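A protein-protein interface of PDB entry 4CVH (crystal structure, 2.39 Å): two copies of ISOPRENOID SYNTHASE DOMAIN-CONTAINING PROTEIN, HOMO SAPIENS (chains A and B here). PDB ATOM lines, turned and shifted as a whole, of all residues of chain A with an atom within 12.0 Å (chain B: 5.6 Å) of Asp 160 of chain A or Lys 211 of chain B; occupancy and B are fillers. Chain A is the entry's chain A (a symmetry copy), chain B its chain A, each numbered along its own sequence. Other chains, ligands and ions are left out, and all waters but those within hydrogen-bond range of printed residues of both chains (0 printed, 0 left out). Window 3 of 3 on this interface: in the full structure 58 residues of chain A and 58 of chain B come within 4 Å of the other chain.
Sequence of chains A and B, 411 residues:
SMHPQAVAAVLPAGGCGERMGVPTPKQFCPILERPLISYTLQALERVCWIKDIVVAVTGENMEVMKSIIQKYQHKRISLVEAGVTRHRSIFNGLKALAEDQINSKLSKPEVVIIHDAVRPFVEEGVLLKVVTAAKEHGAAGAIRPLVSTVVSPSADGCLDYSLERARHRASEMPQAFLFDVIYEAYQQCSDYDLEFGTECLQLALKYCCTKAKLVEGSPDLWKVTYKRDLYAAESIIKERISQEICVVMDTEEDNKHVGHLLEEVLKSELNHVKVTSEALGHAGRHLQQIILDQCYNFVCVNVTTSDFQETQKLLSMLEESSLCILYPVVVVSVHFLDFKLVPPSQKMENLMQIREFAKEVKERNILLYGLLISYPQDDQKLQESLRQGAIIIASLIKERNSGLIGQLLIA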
ATOM      1  N   THR A 149       2.026 -20.200  14.336  1.00  0.00           N
ATOM      2  CA  THR A 149       2.757 -18.995  13.942  1.00  0.00           C
ATOM      3  C   THR A 149       4.098 -18.980  14.670  1.00  0.00           C
ATOM      4  O   THR A 149       4.198 -19.416  15.823  1.00  0.00           O
ATOM      5  CB  THR A 149       1.957 -17.717  14.249  1.00  0.00           C
ATOM      6  OG1 THR A 149       0.807 -17.672  13.396  1.00  0.00           O
ATOM      7  CG2 THR A 149       2.800 -16.455  14.012  1.00  0.00           C
ATOM      8  N   VAL A 150       5.124 -18.504  13.978  1.00  0.00           N
ATOM      9  CA  VAL A 150       6.459 -18.390  14.546  1.00  0.00           C
ATOM     10  C   VAL A 150       6.706 -16.955  14.960  1.00  0.00           C
ATOM     11  O   VAL A 150       6.376 -16.040  14.214  1.00  0.00           O
ATOM     12  CB  VAL A 150       7.533 -18.799  13.540  1.00  0.00           C
ATOM     13  CG1 VAL A 150       8.916 -18.668  14.160  1.00  0.00           C
ATOM     14  CG2 VAL A 150       7.294 -20.226  13.096  1.00  0.00           C
ATOM     15  N   VAL A 151       7.297 -16.778  16.142  1.00  0.00           N
ATOM     16  CA  VAL A 151       7.548 -15.460  16.711  1.00  0.00           C
ATOM     17  C   VAL A 151       8.966 -15.351  17.237  1.00  0.00           C
ATOM     18  O   VAL A 151       9.615 -16.354  17.502  1.00  0.00           O
ATOM     19  CB  VAL A 151       6.588 -15.115  17.868  1.00  0.00           C
ATOM     20  CG1 VAL A 151       5.147 -15.119  17.379  1.00  0.00           C
ATOM     21  CG2 VAL A 151       6.767 -16.062  19.047  1.00  0.00           C
ATOM     22  N   SER A 152       9.431 -14.114  17.373  1.00  0.00           N
ATOM     23  CA  SER A 152      10.763 -13.821  17.900  1.00  0.00           C
ATOM     24  C   SER A 152      10.602 -13.065  19.202  1.00  0.00           C
ATOM     25  O   SER A 152       9.979 -12.009  19.206  1.00  0.00           O
ATOM     26  CB  SER A 152      11.549 -12.961  16.912  1.00  0.00           C
ATOM     27  OG  SER A 152      12.845 -12.704  17.405  1.00  0.00           O
ATOM     28  N   PRO A 153      11.131 -13.609  20.312  1.00  0.00           N
ATOM     29  CA  PRO A 153      11.078 -12.906  21.597  1.00  0.00           C
ATOM     30  C   PRO A 153      12.196 -11.886  21.762  1.00  0.00           C
ATOM     31  O   PRO A 153      13.244 -12.006  21.139  1.00  0.00           O
ATOM     32  CB  PRO A 153      11.238 -14.029  22.623  1.00  0.00           C
ATOM     33  CG  PRO A 153      11.988 -15.096  21.913  1.00  0.00           C
ATOM     34  CD  PRO A 153      11.721 -14.953  20.441  1.00  0.00           C
ATOM     35  N   SER A 154      11.949 -10.876  22.584  1.00  0.00           N
ATOM     36  CA  SER A 154      12.977  -9.925  22.979  1.00  0.00           C
ATOM     37  C   SER A 154      13.681 -10.496  24.208  1.00  0.00           C
ATOM     38  O   SER A 154      13.219 -11.498  24.779  1.00  0.00           O
ATOM     39  CB  SER A 154      12.347  -8.576  23.313  1.00  0.00           C
ATOM     40  OG  SER A 154      11.645  -8.645  24.539  1.00  0.00           O
ATOM     41  N   ALA A 155      14.775  -9.854  24.625  1.00  0.00           N
ATOM     42  CA  ALA A 155      15.552 -10.309  25.792  1.00  0.00           C
ATOM     43  C   ALA A 155      14.688 -10.457  27.045  1.00  0.00           C
ATOM     44  O   ALA A 155      14.841 -11.424  27.792  1.00  0.00           O
ATOM     45  CB  ALA A 155      16.713  -9.361  26.064  1.00  0.00           C
ATOM     46  N   ASP A 156      13.763  -9.517  27.255  1.00  0.00           N
ATOM     47  CA  ASP A 156      12.848  -9.579  28.407  1.00  0.00           C
ATOM     48  C   ASP A 156      11.622 -10.495  28.183  1.00  0.00           C
ATOM     49  O   ASP A 156      10.663 -10.458  28.962  1.00  0.00           O
ATOM     50  CB  ASP A 156      12.419  -8.164  28.856  1.00  0.00           C
ATOM     51  CG  ASP A 156      11.735  -7.363  27.753  1.00  0.00           C
ATOM     52  OD1 ASP A 156      12.270  -7.319  26.626  1.00  0.00           O
ATOM     53  OD2 ASP A 156      10.674  -6.757  28.021  1.00  0.00           O
ATOM     54  N   GLY A 157      11.664 -11.326  27.138  1.00  0.00           N
ATOM     55  CA  GLY A 157      10.616 -12.317  26.881  1.00  0.00           C
ATOM     56  C   GLY A 157       9.292 -11.736  26.420  1.00  0.00           C
ATOM     57  O   GLY A 157       8.233 -12.206  26.829  1.00  0.00           O
ATOM     58  N   CYS A 158       9.354 -10.710  25.576  1.00  0.00           N
ATOM     59  CA  CYS A 158       8.163 -10.114  24.986  1.00  0.00           C
ATOM     60  C   CYS A 158       8.198 -10.211  23.466  1.00  0.00           C
ATOM     61  O   CYS A 158       9.257 -10.415  22.861  1.00  0.00           O
ATOM     62  CB  CYS A 158       8.015  -8.664  25.429  1.00  0.00           C
ATOM     63  SG  CYS A 158       7.591  -8.533  27.183  1.00  0.00           S
ATOM     64  N   LEU A 159       7.026 -10.091  22.855  1.00  0.00           N
ATOM     65  CA  LEU A 159       6.904 -10.249  21.420  1.00  0.00           C
ATOM     66  C   LEU A 159       7.674  -9.169  20.691  1.00  0.00           C
ATOM     67  O   LEU A 159       7.404  -7.984  20.867  1.00  0.00           O
ATOM     68  CB  LEU A 159       5.438 -10.182  20.991  1.00  0.00           C
ATOM     69  CG  LEU A 159       5.186 -10.279  19.488  1.00  0.00           C
ATOM     70  CD1 LEU A 159       5.731 -11.584  18.920  1.00  0.00           C
ATOM     71  CD2 LEU A 159       3.701 -10.149  19.208  1.00  0.00           C
ATOM     72  N   ASP A 160       8.606  -9.588  19.846  1.00  0.00           N
ATOM     73  CA  ASP A 160       9.407  -8.667  19.059  1.00  0.00           C
ATOM     74  C   ASP A 160       8.764  -8.538  17.687  1.00  0.00           C
ATOM     75  O   ASP A 160       8.427  -7.435  17.251  1.00  0.00           O
ATOM     76  CB  ASP A 160      10.839  -9.201  18.949  1.00  0.00           C
ATOM     77  CG  ASP A 160      11.864  -8.156  19.202  1.00  0.00           C
ATOM     78  OD1 ASP A 160      11.754  -7.483  20.243  1.00  0.00           O
ATOM     79  OD2 ASP A 160      12.784  -8.020  18.373  1.00  0.00           O
ATOM     80  N   TYR A 161       8.591  -9.673  17.009  1.00  0.00           N
ATOM     81  CA  TYR A 161       7.841  -9.720  15.748  1.00  0.00           C
ATOM     82  C   TYR A 161       7.279 -11.130  15.503  1.00  0.00           C
ATOM     83  O   TYR A 161       7.664 -12.086  16.188  1.00  0.00           O
ATOM     84  CB  TYR A 161       8.707  -9.229  14.563  1.00  0.00           C
ATOM     85  CG  TYR A 161       9.939 -10.061  14.299  1.00  0.00           C
ATOM     86  CD1 TYR A 161       9.862 -11.214  13.526  1.00  0.00           C
ATOM     87  CD2 TYR A 161      11.186  -9.704  14.823  1.00  0.00           C
ATOM     88  CE1 TYR A 161      10.976 -12.004  13.294  1.00  0.00           C
ATOM     89  CE2 TYR A 161      12.312 -10.487  14.587  1.00  0.00           C
ATOM     90  CZ  TYR A 161      12.200 -11.638  13.819  1.00  0.00           C
ATOM     91  OH  TYR A 161      13.287 -12.443  13.564  1.00  0.00           O
ATOM     92  N   SER A 162       6.341 -11.219  14.555  1.00  0.00           N
ATOM     93  CA  SER A 162       5.761 -12.477  14.077  1.00  0.00           C
ATOM     94  C   SER A 162       6.115 -12.695  12.621  1.00  0.00           C
ATOM     95  O   SER A 162       6.218 -11.747  11.857  1.00  0.00           O
ATOM     96  CB  SER A 162       4.238 -12.452  14.165  1.00  0.00           C
ATOM     97  OG  SER A 162       3.807 -12.498  15.505  1.00  0.00           O
ATOM     98  N   LEU A 163       6.254 -13.948  12.222  1.00  0.00           N
ATOM     99  CA  LEU A 163       6.581 -14.250  10.843  1.00  0.00           C
ATOM    100  C   LEU A 163       5.332 -14.627  10.083  1.00  0.00           C
ATOM    101  O   LEU A 163       4.403 -15.211  10.639  1.00  0.00           O
ATOM    102  CB  LEU A 163       7.624 -15.359  10.759  1.00  0.00           C
ATOM    103  CG  LEU A 163       8.992 -14.955  11.308  1.00  0.00           C
ATOM    104  CD1 LEU A 163       9.855 -16.192  11.432  1.00  0.00           C
ATOM    105  CD2 LEU A 163       9.682 -13.919  10.429  1.00  0.00           C
ATOM    106  N   GLU A 164       5.322 -14.279   8.804  1.00  0.00           N
ATOM    107  CA  GLU A 164       4.209 -14.587   7.941  1.00  0.00           C
ATOM    108  C   GLU A 164       4.206 -16.097   7.707  1.00  0.00           C
ATOM    109  O   GLU A 164       5.151 -16.656   7.153  1.00  0.00           O
ATOM    110  CB  GLU A 164       4.321 -13.817   6.625  1.00  0.00           C
ATOM    111  CG  GLU A 164       2.998 -13.704   5.878  1.00  0.00           C
ATOM    112  CD  GLU A 164       3.149 -13.131   4.479  1.00  0.00           C
ATOM    113  OE1 GLU A 164       4.173 -12.465   4.197  1.00  0.00           O
ATOM    114  OE2 GLU A 164       2.233 -13.350   3.662  1.00  0.00           O
ATOM    115  N   HIS B 137       0.743  -6.465  31.229  1.00  0.00           N
ATOM    116  CA  HIS B 137       1.305  -6.048  29.928  1.00  0.00           C
ATOM    117  C   HIS B 137       0.288  -5.669  28.842  1.00  0.00           C
ATOM    118  O   HIS B 137       0.668  -5.126  27.807  1.00  0.00           O
ATOM    119  CB  HIS B 137       2.191  -7.156  29.354  1.00  0.00           C
ATOM    120  CG  HIS B 137       3.501  -7.330  30.053  1.00  0.00           C
ATOM    121  ND1 HIS B 137       3.670  -8.185  31.123  1.00  0.00           N
ATOM    122  CD2 HIS B 137       4.721  -6.802  29.799  1.00  0.00           C
ATOM    123  CE1 HIS B 137       4.933  -8.160  31.510  1.00  0.00           C
ATOM    124  NE2 HIS B 137       5.591  -7.327  30.724  1.00  0.00           N
ATOM    125  N   ALA B 139      -1.274  -7.811  26.896  1.00  0.00           N
ATOM    126  CA  ALA B 139      -1.400  -9.000  26.074  1.00  0.00           C
ATOM    127  C   ALA B 139      -0.403 -10.037  26.541  1.00  0.00           C
ATOM    128  O   ALA B 139       0.654  -9.692  27.090  1.00  0.00           O
ATOM    129  CB  ALA B 139      -1.134  -8.661  24.620  1.00  0.00           C
ATOM    130  N   GLN B 202      -0.008 -10.204  17.307  1.00  0.00           N
ATOM    131  CA  GLN B 202       0.564  -9.317  16.292  1.00  0.00           C
ATOM    132  C   GLN B 202      -0.392  -8.170  16.042  1.00  0.00           C
ATOM    133  O   GLN B 202       0.057  -7.075  15.767  1.00  0.00           O
ATOM    134  CB  GLN B 202       0.860 -10.046  14.978  1.00  0.00           C
ATOM    135  CG  GLN B 202       1.635  -9.230  13.943  1.00  0.00           C
ATOM    136  CD  GLN B 202       2.959  -8.675  14.477  1.00  0.00           C
ATOM    137  OE1 GLN B 202       3.804  -9.413  14.985  1.00  0.00           O
ATOM    138  NE2 GLN B 202       3.138  -7.370  14.366  1.00  0.00           N
ATOM    139  N   LEU B 205       0.211  -5.754  18.880  1.00  0.00           N
ATOM    140  CA  LEU B 205       1.461  -5.043  18.625  1.00  0.00           C
ATOM    141  C   LEU B 205       1.345  -3.964  17.515  1.00  0.00           C
ATOM    142  O   LEU B 205       1.818  -2.857  17.680  1.00  0.00           O
ATOM    143  CB  LEU B 205       2.577  -6.041  18.305  1.00  0.00           C
ATOM    144  CG  LEU B 205       3.949  -5.435  17.965  1.00  0.00           C
ATOM    145  CD1 LEU B 205       4.437  -4.531  19.080  1.00  0.00           C
ATOM    146  CD2 LEU B 205       4.970  -6.527  17.690  1.00  0.00           C
ATOM    147  N   CYS B 209       0.393  -0.814  19.812  1.00  0.00           N
ATOM    148  CA  CYS B 209       1.739  -0.815  20.390  1.00  0.00           C
ATOM    149  C   CYS B 209       1.755  -1.506  21.751  1.00  0.00           C
ATOM    150  O   CYS B 209       2.209  -0.941  22.744  1.00  0.00           O
ATOM    151  CB  CYS B 209       2.268   0.618  20.493  1.00  0.00           C
ATOM    152  SG  CYS B 209       2.287   1.467  18.899  1.00  0.00           S
ATOM    153  N   THR B 210       1.218  -2.720  21.778  1.00  0.00           N
ATOM    154  CA  THR B 210       1.228  -3.570  22.957  1.00  0.00           C
ATOM    155  C   THR B 210       2.154  -4.748  22.695  1.00  0.00           C
ATOM    156  O   THR B 210       1.861  -5.585  21.851  1.00  0.00           O
ATOM    157  CB  THR B 210      -0.176  -4.110  23.254  1.00  0.00           C
ATOM    158  OG1 THR B 210      -1.085  -3.013  23.409  1.00  0.00           O
ATOM    159  CG2 THR B 210      -0.173  -4.961  24.525  1.00  0.00           C
ATOM    160  N   LYS B 211       3.271  -4.800  23.412  1.00  0.00           N
ATOM    161  CA  LYS B 211       4.223  -5.899  23.285  1.00  0.00           C
ATOM    162  C   LYS B 211       3.834  -7.031  24.235  1.00  0.00           C
ATOM    163  O   LYS B 211       4.007  -6.913  25.449  1.00  0.00           O
ATOM    164  CB  LYS B 211       5.652  -5.413  23.574  1.00  0.00           C
ATOM    165  CG  LYS B 211       6.245  -4.584  22.439  1.00  0.00           C
ATOM    166  CD  LYS B 211       7.735  -4.310  22.598  1.00  0.00           C
ATOM    167  CE  LYS B 211       8.552  -5.592  22.708  1.00  0.00           C
ATOM    168  NZ  LYS B 211       9.788  -5.568  21.882  1.00  0.00           N
ATOM    169  N   ALA B 212       3.313  -8.127  23.684  1.00  0.00           N
ATOM    170  CA  ALA B 212       2.791  -9.216  24.511  1.00  0.00           C
ATOM    171  C   ALA B 212       3.890  -9.911  25.305  1.00  0.00           C
ATOM    172  O   ALA B 212       5.021 -10.048  24.827  1.00  0.00           O
ATOM    173  CB  ALA B 212       2.042 -10.235  23.657  1.00  0.00           C
ATOM    174  N   LYS B 213       3.550 -10.348  26.514  1.00  0.00           N
ATOM    175  CA  LYS B 213       4.450 -11.185  27.311  1.00  0.00           C
ATOM    176  C   LYS B 213       4.339 -12.645  26.860  1.00  0.00           C
ATOM    177  O   LYS B 213       3.241 -13.203  26.790  1.00  0.00           O
ATOM    178  CB  LYS B 213       4.115 -11.078  28.804  1.00  0.00           C
ATOM    179  CG  LYS B 213       5.048 -11.849  29.732  1.00  0.00           C
ATOM    180  CD  LYS B 213       6.432 -11.207  29.798  1.00  0.00           C
ATOM    181  CE  LYS B 213       7.432 -12.031  30.597  1.00  0.00           C
ATOM    182  NZ  LYS B 213       8.035 -13.126  29.786  1.00  0.00           N
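The side-chain hydroxyl (OG) of Ser 162 of chain A lies within hydrogen-bond range of the side-chain amide oxygen (OE1) of Gln 202 of chain B (3.1 Å).
The side-chain carboxylate (OD1) of Asp 160 of chain A is in salt-bridge range of the side-chain amino group (NZ) of Lys 211 of chain B (3.2 Å).
The backbone carbonyl oxygen (O) of Ala 212 of chain B lies within hydrogen-bond range of the backbone NH (N) of Leu 159 of chain A (2.8 Å).
The side-chain amino group (NZ) of Lys 213 of chain B lies within hydrogen-bond range of the backbone carbonyl oxygen (O) of Gly 157 of chain A, at 3.1 Å.
O of Ala 139 of chain B sits at hydrogen-bond distance from N of Lys 213 of chain B, at 3.0 Å.
The backbone carbonyl oxygen of Thr 210 of chain B sits close to the backbone NH of Leu 205 of chain B.
The backbone NH of Ser 152 of chain A is in hydrogen-bond range of the backbone carbonyl oxygen of Tyr 161 of chain A.
The side-chain hydroxyl (OG) of Ser 154 of chain A is in hydrogen-bond range of the side-chain carboxylate (OD1) of Asp 156 of chain A, at 2.6 Å.
The backbone NH (N) of Cys 158 of chain A lies within hydrogen-bond range of the side-chain hydroxyl (OG) of Ser 154 of chain A, 3.3 Å away.
The side-chain carboxylate (OD2) of Asp 156 of chain A sits at hydrogen-bond distance from the side-chain sulfur (SG) of Cys 158 of chain A (3.7 Å).
Among the printed residues, pairs that only touch across the chains: Cys 158 of chain A with Ala 212 of chain B, Leu 159 of chain A with Lys 211 of chain B, Asp 160 of chain A with Leu 205 of chain B, Asp 156 of chain A with Lys 213 of chain B, Tyr 161 of chain A with Gln 202 of chain B and Cys 158 of chain A with Lys 213 of chain B.
Printed residues of chain B within 4 Å of Cys 158 of chain A: Ala 212 (3.1 Å) and Lys 213 (3.9 Å).
Asp 160 of chain A touches just these residues of chain B: Leu 205 (3.6 Å) and Lys 211 (3.2 Å).
Of the printed residues of chain B, Tyr 161 of chain A touches Gln 202.
Printed residues of chain B within 4 Å of Ser 162 of chain A: Gln 202.
No residue of chain A comes within 4 Å of His 137 of chain B.
No residue of chain A comes within 4 Å of Ala 139 of chain B.
Of chain A, only Asp 160 comes within 4 Å of Leu 205 of chain B.
No residue of chain A comes within 4 Å of Cys 209 of chain B.
Of chain A, only Leu 159 and Asp 160 come within 4 Å of Lys 211 of chain B.
Of chain A, only Cys 158 and Leu 159 come within 4 Å of Ala 212 of chain B.
The nearest residue of chain B that does not touch Asp 160 of chain A is Gln 202 of chain B (5.5 Å).
The nearest residue of chain A that does not touch Lys 211 of chain B is Cys 158 of chain A (4.1 Å).
Along chain B the printed residues that touch a printed residue of chain A span positions 202 to 213.
Among the printed residues, 10 pairs touch across the chains.
Among the printed residues, Asp or Glu carboxylates within 4 Å of a Lys or Arg side-chain nitrogen of the other chain: Asp 160 of chain A with Lys 211 of chain B (3.2 Å).
No position is printed for both chains.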
